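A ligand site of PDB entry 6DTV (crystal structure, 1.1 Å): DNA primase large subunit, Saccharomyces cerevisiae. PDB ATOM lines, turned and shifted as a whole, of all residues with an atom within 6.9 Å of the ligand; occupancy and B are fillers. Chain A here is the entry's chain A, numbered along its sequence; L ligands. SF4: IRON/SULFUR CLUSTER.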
ATOM      1  N   PRO A  19     -28.202  19.273 -16.739  1.00  0.00           N
ATOM      2  CA  PRO A  19     -26.916  19.160 -16.044  1.00  0.00           C
ATOM      3  C   PRO A  19     -27.102  18.359 -14.767  1.00  0.00           C
ATOM      4  O   PRO A  19     -28.214  18.090 -14.303  1.00  0.00           O
ATOM      5  CB  PRO A  19     -26.517  20.609 -15.781  1.00  0.00           C
ATOM      6  CG  PRO A  19     -27.852  21.306 -15.652  1.00  0.00           C
ATOM      7  CD  PRO A  19     -28.771  20.622 -16.628  1.00  0.00           C
ATOM      8  N   LEU A  20     -25.973  18.045 -14.137  1.00  0.00           N
ATOM      9  CA  LEU A  20     -26.013  17.136 -13.002  1.00  0.00           C
ATOM     10  C   LEU A  20     -26.845  17.656 -11.839  1.00  0.00           C
ATOM     11  O   LEU A  20     -27.483  16.858 -11.136  1.00  0.00           O
ATOM     12  CB  LEU A  20     -24.598  16.816 -12.566  1.00  0.00           C
ATOM     13  CG  LEU A  20     -24.370  15.619 -11.748  1.00  0.00           C
ATOM     14  CD1 LEU A  20     -25.075  14.409 -12.249  1.00  0.00           C
ATOM     15  CD2 LEU A  20     -22.869  15.438 -11.755  1.00  0.00           C
ATOM     16  N   CYS A  21     -26.808  18.963 -11.561  1.00  0.00           N
ATOM     17  CA  CYS A  21     -27.602  19.488 -10.453  1.00  0.00           C
ATOM     18  C   CYS A  21     -29.103  19.216 -10.662  1.00  0.00           C
ATOM     19  O   CYS A  21     -29.810  18.810  -9.737  1.00  0.00           O
ATOM     20  CB  CYS A  21     -27.373  20.967 -10.204  1.00  0.00           C
ATOM     21  SG  CYS A  21     -27.620  22.031 -11.694  1.00  0.00           S
ATOM     22  N   ILE A  22     -29.598  19.435 -11.879  1.00  0.00           N
ATOM     23  CA  ILE A  22     -31.004  19.235 -12.197  1.00  0.00           C
ATOM     24  C   ILE A  22     -31.334  17.768 -12.194  1.00  0.00           C
ATOM     25  O   ILE A  22     -32.386  17.365 -11.675  1.00  0.00           O
ATOM     26  CB  ILE A  22     -31.357  19.949 -13.516  1.00  0.00           C
ATOM     27  CG1 ILE A  22     -31.126  21.445 -13.432  1.00  0.00           C
ATOM     28  CG2 ILE A  22     -32.763  19.627 -13.930  1.00  0.00           C
ATOM     29  CD1 ILE A  22     -31.797  22.171 -12.277  1.00  0.00           C
ATOM     30  N   GLN A  42     -34.640  25.887  -6.784  1.00  0.00           N
ATOM     31  CA  GLN A  42     -33.665  25.656  -7.852  1.00  0.00           C
ATOM     32  C   GLN A  42     -34.328  24.938  -9.024  1.00  0.00           C
ATOM     33  O   GLN A  42     -34.183  25.337 -10.174  1.00  0.00           O
ATOM     34  CB  GLN A  42     -32.496  24.842  -7.303  1.00  0.00           C
ATOM     35  CG  GLN A  42     -31.341  24.712  -8.292  1.00  0.00           C
ATOM     36  CD  GLN A  42     -30.100  24.093  -7.668  1.00  0.00           C
ATOM     37  OE1 GLN A  42     -29.934  24.112  -6.453  1.00  0.00           O
ATOM     38  NE2 GLN A  42     -29.226  23.550  -8.498  1.00  0.00           N
ATOM     39  N   ASP A 101     -28.406  31.018 -11.812  1.00  0.00           N
ATOM     40  CA  ASP A 101     -27.156  30.656 -12.484  1.00  0.00           C
ATOM     41  C   ASP A 101     -26.237  29.875 -11.547  1.00  0.00           C
ATOM     42  O   ASP A 101     -26.548  29.662 -10.388  1.00  0.00           O
ATOM     43  CB  ASP A 101     -26.510  31.902 -13.114  1.00  0.00           C
ATOM     44  CG  ASP A 101     -25.964  32.899 -12.162  1.00  0.00           C
ATOM     45  OD1 ASP A 101     -25.908  32.655 -10.990  1.00  0.00           O
ATOM     46  OD2 ASP A 101     -25.532  33.952 -12.681  1.00  0.00           O
ATOM     47  N   CYS A 102     -25.106  29.385 -12.080  1.00  0.00           N
ATOM     48  CA  CYS A 102     -24.263  28.521 -11.270  1.00  0.00           C
ATOM     49  C   CYS A 102     -23.704  29.276 -10.084  1.00  0.00           C
ATOM     50  O   CYS A 102     -23.604  28.724  -8.981  1.00  0.00           O
ATOM     51  CB  CYS A 102     -23.120  27.922 -12.066  1.00  0.00           C
ATOM     52  SG  CYS A 102     -23.719  26.907 -13.475  1.00  0.00           S
ATOM     53  N   HIS A 103     -23.284  30.525 -10.284  1.00  0.00           N
ATOM     54  CA  HIS A 103     -22.743  31.271  -9.159  1.00  0.00           C
ATOM     55  C   HIS A 103     -23.783  31.442  -8.057  1.00  0.00           C
ATOM     56  O   HIS A 103     -23.483  31.280  -6.875  1.00  0.00           O
ATOM     57  CB  HIS A 103     -22.255  32.616  -9.632  1.00  0.00           C
ATOM     58  CG  HIS A 103     -21.568  33.418  -8.570  1.00  0.00           C
ATOM     59  ND1 HIS A 103     -20.229  33.316  -8.282  1.00  0.00           N
ATOM     60  CD2 HIS A 103     -22.075  34.324  -7.698  1.00  0.00           C
ATOM     61  CE1 HIS A 103     -19.934  34.150  -7.289  1.00  0.00           C
ATOM     62  NE2 HIS A 103     -21.033  34.767  -6.921  1.00  0.00           N
ATOM     63  N   ILE A 105     -26.367  29.366  -7.497  1.00  0.00           N
ATOM     64  CA  ILE A 105     -26.517  28.033  -6.890  1.00  0.00           C
ATOM     65  C   ILE A 105     -25.427  27.767  -5.882  1.00  0.00           C
ATOM     66  O   ILE A 105     -25.684  27.314  -4.764  1.00  0.00           O
ATOM     67  CB  ILE A 105     -26.556  26.996  -8.006  1.00  0.00           C
ATOM     68  CG1 ILE A 105     -27.913  27.078  -8.697  1.00  0.00           C
ATOM     69  CG2 ILE A 105     -26.341  25.614  -7.476  1.00  0.00           C
ATOM     70  CD1 ILE A 105     -27.917  26.421 -10.073  1.00  0.00           C
ATOM     71  N   LEU A 106     -24.176  27.997  -6.292  1.00  0.00           N
ATOM     72  CA  LEU A 106     -23.032  27.705  -5.438  1.00  0.00           C
ATOM     73  C   LEU A 106     -23.039  28.579  -4.188  1.00  0.00           C
ATOM     74  O   LEU A 106     -22.494  28.184  -3.154  1.00  0.00           O
ATOM     75  CB  LEU A 106     -21.732  27.895  -6.257  1.00  0.00           C
ATOM     76  CG  LEU A 106     -21.461  26.779  -7.263  1.00  0.00           C
ATOM     77  CD1 LEU A 106     -20.484  27.220  -8.327  1.00  0.00           C
ATOM     78  CD2 LEU A 106     -21.012  25.520  -6.591  1.00  0.00           C
ATOM     79  N   GLY A 118     -27.917  22.644  -4.864  1.00  0.00           N
ATOM     80  CA  GLY A 118     -26.479  22.848  -4.935  1.00  0.00           C
ATOM     81  C   GLY A 118     -25.914  22.346  -6.249  1.00  0.00           C
ATOM     82  O   GLY A 118     -26.602  22.271  -7.276  1.00  0.00           O
ATOM     83  N   CYS A 119     -24.612  22.038  -6.217  1.00  0.00           N
ATOM     84  CA  CYS A 119     -23.844  21.629  -7.404  1.00  0.00           C
ATOM     85  C   CYS A 119     -23.172  20.297  -7.077  1.00  0.00           C
ATOM     86  O   CYS A 119     -22.256  20.278  -6.244  1.00  0.00           O
ATOM     87  CB  CYS A 119     -22.805  22.681  -7.773  1.00  0.00           C
ATOM     88  SG  CYS A 119     -21.780  22.133  -9.160  1.00  0.00           S
ATOM     89  N   PRO A 120     -23.565  19.199  -7.714  1.00  0.00           N
ATOM     90  CA  PRO A 120     -22.940  17.924  -7.388  1.00  0.00           C
ATOM     91  C   PRO A 120     -21.420  17.889  -7.546  1.00  0.00           C
ATOM     92  O   PRO A 120     -20.780  17.080  -6.863  1.00  0.00           O
ATOM     93  CB  PRO A 120     -23.632  16.929  -8.346  1.00  0.00           C
ATOM     94  CG  PRO A 120     -25.050  17.557  -8.487  1.00  0.00           C
ATOM     95  CD  PRO A 120     -24.755  19.031  -8.565  1.00  0.00           C
ATOM     96  N   PHE A 121     -20.860  18.654  -8.452  1.00  0.00           N
ATOM     97  CA  PHE A 121     -19.410  18.630  -8.611  1.00  0.00           C
ATOM     98  C   PHE A 121     -18.694  19.071  -7.356  1.00  0.00           C
ATOM     99  O   PHE A 121     -17.550  18.668  -7.127  1.00  0.00           O
ATOM    100  CB  PHE A 121     -19.029  19.475  -9.813  1.00  0.00           C
ATOM    101  CG  PHE A 121     -19.504  18.898 -11.102  1.00  0.00           C
ATOM    102  CD1 PHE A 121     -18.932  17.756 -11.639  1.00  0.00           C
ATOM    103  CD2 PHE A 121     -20.590  19.422 -11.791  1.00  0.00           C
ATOM    104  CE1 PHE A 121     -19.392  17.203 -12.818  1.00  0.00           C
ATOM    105  CE2 PHE A 121     -21.042  18.854 -12.956  1.00  0.00           C
ATOM    106  CZ  PHE A 121     -20.475  17.766 -13.489  1.00  0.00           C
ATOM    107  N   ARG A 122     -19.331  19.914  -6.565  1.00  0.00           N
ATOM    108  CA  ARG A 122     -18.868  20.291  -5.255  1.00  0.00           C
ATOM    109  C   ARG A 122     -19.356  19.396  -4.159  1.00  0.00           C
ATOM    110  O   ARG A 122     -18.615  19.092  -3.218  1.00  0.00           O
ATOM    111  CB  ARG A 122     -19.278  21.733  -4.920  1.00  0.00           C
ATOM    112  CG  ARG A 122     -18.798  22.199  -3.564  1.00  0.00           C
ATOM    113  CD  ARG A 122     -19.382  23.530  -3.201  1.00  0.00           C
ATOM    114  NE  ARG A 122     -20.805  23.376  -2.986  1.00  0.00           N
ATOM    115  CZ  ARG A 122     -21.727  24.331  -2.902  1.00  0.00           C
ATOM    116  NH1 ARG A 122     -21.367  25.605  -2.898  1.00  0.00           N
ATOM    117  NH2 ARG A 122     -23.006  23.983  -2.807  1.00  0.00           N
ATOM    118  N   TYR A 155     -15.796  24.069 -10.362  1.00  0.00           N
ATOM    119  CA  TYR A 155     -17.003  23.251 -10.574  1.00  0.00           C
ATOM    120  C   TYR A 155     -17.626  23.465 -11.941  1.00  0.00           C
ATOM    121  O   TYR A 155     -18.078  22.519 -12.558  1.00  0.00           O
ATOM    122  CB  TYR A 155     -18.009  23.493  -9.426  1.00  0.00           C
ATOM    123  CG  TYR A 155     -17.371  23.307  -8.099  1.00  0.00           C
ATOM    124  CD1 TYR A 155     -16.736  22.134  -7.754  1.00  0.00           C
ATOM    125  CD2 TYR A 155     -17.332  24.369  -7.206  1.00  0.00           C
ATOM    126  CE1 TYR A 155     -16.037  22.013  -6.546  1.00  0.00           C
ATOM    127  CE2 TYR A 155     -16.682  24.250  -5.965  1.00  0.00           C
ATOM    128  CZ  TYR A 155     -16.030  23.076  -5.657  1.00  0.00           C
ATOM    129  OH  TYR A 155     -15.366  22.947  -4.474  1.00  0.00           O
ATOM    130  N   THR A 156     -17.677  24.713 -12.426  1.00  0.00           N
ATOM    131  CA  THR A 156     -18.273  24.965 -13.721  1.00  0.00           C
ATOM    132  C   THR A 156     -17.397  24.444 -14.852  1.00  0.00           C
ATOM    133  O   THR A 156     -17.922  24.101 -15.900  1.00  0.00           O
ATOM    134  CB  THR A 156     -18.619  26.447 -13.896  1.00  0.00           C
ATOM    135  OG1 THR A 156     -17.425  27.243 -13.894  1.00  0.00           O
ATOM    136  CG2 THR A 156     -19.583  26.939 -12.838  1.00  0.00           C
ATOM    137  N   ILE A 157     -16.076  24.374 -14.643  1.00  0.00           N
ATOM    138  CA  ILE A 157     -15.224  23.722 -15.624  1.00  0.00           C
ATOM    139  C   ILE A 157     -15.469  22.230 -15.643  1.00  0.00           C
ATOM    140  O   ILE A 157     -15.520  21.622 -16.718  1.00  0.00           O
ATOM    141  CB  ILE A 157     -13.741  24.069 -15.384  1.00  0.00           C
ATOM    142  CG1 ILE A 157     -13.513  25.567 -15.608  1.00  0.00           C
ATOM    143  CG2 ILE A 157     -12.873  23.241 -16.323  1.00  0.00           C
ATOM    144  CD1 ILE A 157     -12.087  26.015 -15.385  1.00  0.00           C
ATOM    145  N   ALA A 158     -15.624  21.602 -14.456  1.00  0.00           N
ATOM    146  CA  ALA A 158     -15.974  20.205 -14.414  1.00  0.00           C
ATOM    147  C   ALA A 158     -17.250  19.935 -15.204  1.00  0.00           C
ATOM    148  O   ALA A 158     -17.325  18.970 -15.988  1.00  0.00           O
ATOM    149  CB  ALA A 158     -16.121  19.752 -12.973  1.00  0.00           C
ATOM    150  N   CYS A 159     -18.267  20.776 -14.994  1.00  0.00           N
ATOM    151  CA  CYS A 159     -19.542  20.624 -15.666  1.00  0.00           C
ATOM    152  C   CYS A 159     -19.395  20.802 -17.182  1.00  0.00           C
ATOM    153  O   CYS A 159     -19.985  20.043 -17.965  1.00  0.00           O
ATOM    154  CB  CYS A 159     -20.504  21.647 -15.034  1.00  0.00           C
ATOM    155  SG  CYS A 159     -22.198  21.496 -15.598  1.00  0.00           S
ATOM    156  N   THR A 160     -18.568  21.781 -17.601  1.00  0.00           N
ATOM    157  CA  THR A 160     -18.293  21.979 -19.018  1.00  0.00           C
ATOM    158  C   THR A 160     -17.604  20.754 -19.617  1.00  0.00           C
ATOM    159  O   THR A 160     -17.911  20.357 -20.741  1.00  0.00           O
ATOM    160  CB  THR A 160     -17.445  23.224 -19.199  1.00  0.00           C
ATOM    161  OG1 THR A 160     -18.123  24.365 -18.666  1.00  0.00           O
ATOM    162  CG2 THR A 160     -17.202  23.497 -20.627  1.00  0.00           C
ATOM    163  N   ALA A 183     -21.891  30.940 -16.687  1.00  0.00           N
ATOM    164  CA  ALA A 183     -22.211  29.557 -16.336  1.00  0.00           C
ATOM    165  C   ALA A 183     -23.651  29.474 -15.812  1.00  0.00           C
ATOM    166  O   ALA A 183     -24.008  30.187 -14.853  1.00  0.00           O
ATOM    167  CB  ALA A 183     -21.240  29.168 -15.212  1.00  0.00           C
ATOM    168  N   HIS A 184     -24.465  28.607 -16.404  1.00  0.00           N
ATOM    169  CA  HIS A 184     -25.887  28.607 -16.068  1.00  0.00           C
ATOM    170  C   HIS A 184     -26.486  27.252 -16.425  1.00  0.00           C
ATOM    171  O   HIS A 184     -26.302  26.787 -17.559  1.00  0.00           O
ATOM    172  CB  HIS A 184     -26.562  29.729 -16.868  1.00  0.00           C
ATOM    173  CG  HIS A 184     -27.875  30.145 -16.381  1.00  0.00           C
ATOM    174  ND1 HIS A 184     -28.906  29.262 -16.120  1.00  0.00           N
ATOM    175  CD2 HIS A 184     -28.305  31.397 -16.019  1.00  0.00           C
ATOM    176  CE1 HIS A 184     -29.907  30.006 -15.638  1.00  0.00           C
ATOM    177  NE2 HIS A 184     -29.574  31.280 -15.574  1.00  0.00           N
ATOM    178  N   PRO A 185     -27.176  26.607 -15.494  1.00  0.00           N
ATOM    179  CA  PRO A 185     -27.844  25.339 -15.844  1.00  0.00           C
ATOM    180  C   PRO A 185     -28.752  25.421 -17.048  1.00  0.00           C
ATOM    181  O   PRO A 185     -28.869  24.448 -17.804  1.00  0.00           O
ATOM    182  CB  PRO A 185     -28.645  24.979 -14.563  1.00  0.00           C
ATOM    183  CG  PRO A 185     -27.954  25.736 -13.434  1.00  0.00           C
ATOM    184  CD  PRO A 185     -27.454  27.038 -14.118  1.00  0.00           C
ATOM    185  N   ASN A 186     -29.435  26.554 -17.213  1.00  0.00           N
ATOM    186  CA  ASN A 186     -30.322  26.696 -18.366  1.00  0.00           C
ATOM    187  C   ASN A 186     -29.534  26.761 -19.677  1.00  0.00           C
ATOM    188  O   ASN A 186     -30.054  26.364 -20.728  1.00  0.00           O
ATOM    189  CB  ASN A 186     -31.293  27.865 -18.212  1.00  0.00           C
ATOM    190  CG  ASN A 186     -32.328  27.555 -17.167  1.00  0.00           C
ATOM    191  OD1 ASN A 186     -32.098  27.658 -15.966  1.00  0.00           O
ATOM    192  ND2 ASN A 186     -33.488  27.123 -17.633  1.00  0.00           N
ATOM    193  N   TYR A 188     -26.664  25.097 -20.131  1.00  0.00           N
ATOM    194  CA  TYR A 188     -26.362  23.693 -20.387  1.00  0.00           C
ATOM    195  C   TYR A 188     -27.516  23.023 -21.104  1.00  0.00           C
ATOM    196  O   TYR A 188     -27.334  22.372 -22.128  1.00  0.00           O
ATOM    197  CB  TYR A 188     -26.060  23.016 -19.059  1.00  0.00           C
ATOM    198  CG  TYR A 188     -25.461  21.650 -19.128  1.00  0.00           C
ATOM    199  CD1 TYR A 188     -26.150  20.517 -19.567  1.00  0.00           C
ATOM    200  CD2 TYR A 188     -24.149  21.468 -18.637  1.00  0.00           C
ATOM    201  CE1 TYR A 188     -25.584  19.266 -19.536  1.00  0.00           C
ATOM    202  CE2 TYR A 188     -23.603  20.217 -18.596  1.00  0.00           C
ATOM    203  CZ  TYR A 188     -24.281  19.125 -19.040  1.00  0.00           C
ATOM    204  OH  TYR A 188     -23.657  17.911 -18.947  1.00  0.00           O
HETATM  205 FE1  SF4 L   1     -25.484  22.719 -12.168  1.00  0.00          FE
HETATM  206 FE2  SF4 L   1     -23.762  24.788 -12.665  1.00  0.00          FE
HETATM  207 FE3  SF4 L   1     -23.269  22.335 -13.732  1.00  0.00          FE
HETATM  208 FE4  SF4 L   1     -22.981  22.732 -11.036  1.00  0.00          FE
HETATM  209  S1  SF4 L   1     -21.722  23.703 -12.642  1.00  0.00           S
HETATM  210  S2  SF4 L   1     -24.032  20.906 -12.109  1.00  0.00           S
HETATM  211  S3  SF4 L   1     -24.650  24.275 -10.633  1.00  0.00           S
HETATM  212  S4  SF4 L   1     -25.097  23.634 -14.198  1.00  0.00           S
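The side-chain sulfur (SG) of Cys 102 binds an iron atom (FE2) of the ligand (2.3 Å).
The backbone NH of Cys 21 lies close to a sulfur (S2) of the ligand, at 3.4 Å.
An iron atom (FE1) of the ligand is bound by the side-chain sulfur (SG) of Cys 21 (2.3 Å).
FE4 of the ligand is bound by SG of Cys 119 (2.3 Å).
The side-chain sulfur of Cys 159 binds an iron atom (FE3) of the ligand, 2.3 Å away.
N of His 184 sits close to SG of Cys 102, at 3.5 Å.
The backbone carbonyl oxygen (O) of Ala 183 lies within hydrogen-bond range of the backbone NH (N) of Cys 102 (3.1 Å).
N of Phe 121 lies close to SG of Cys 119.
The backbone carbonyl oxygen (O) of Thr 156 lies within hydrogen-bond range of the side-chain hydroxyl (OG1) of Thr 160, 2.8 Å away.
Residues that only touch the ligand: Pro 185 (3.6 Å), Pro 19 (3.7 Å), Phe 121 (3.7 Å), Ile 105 (3.8 Å), Thr 156 (3.8 Å) and Tyr 155 (3.8 Å).
Hydrophobic or aromatic side chains within 4 Å of the ligand: Pro 19, Ile 105, Phe 121 and Pro 185.
Ten residues have an atom within 4 Å of the ligand: Pro 19, Cys 21, Cys 102, Ile 105, Cys 119, Phe 121, Tyr 155, Thr 156, Cys 159 and Pro 185.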
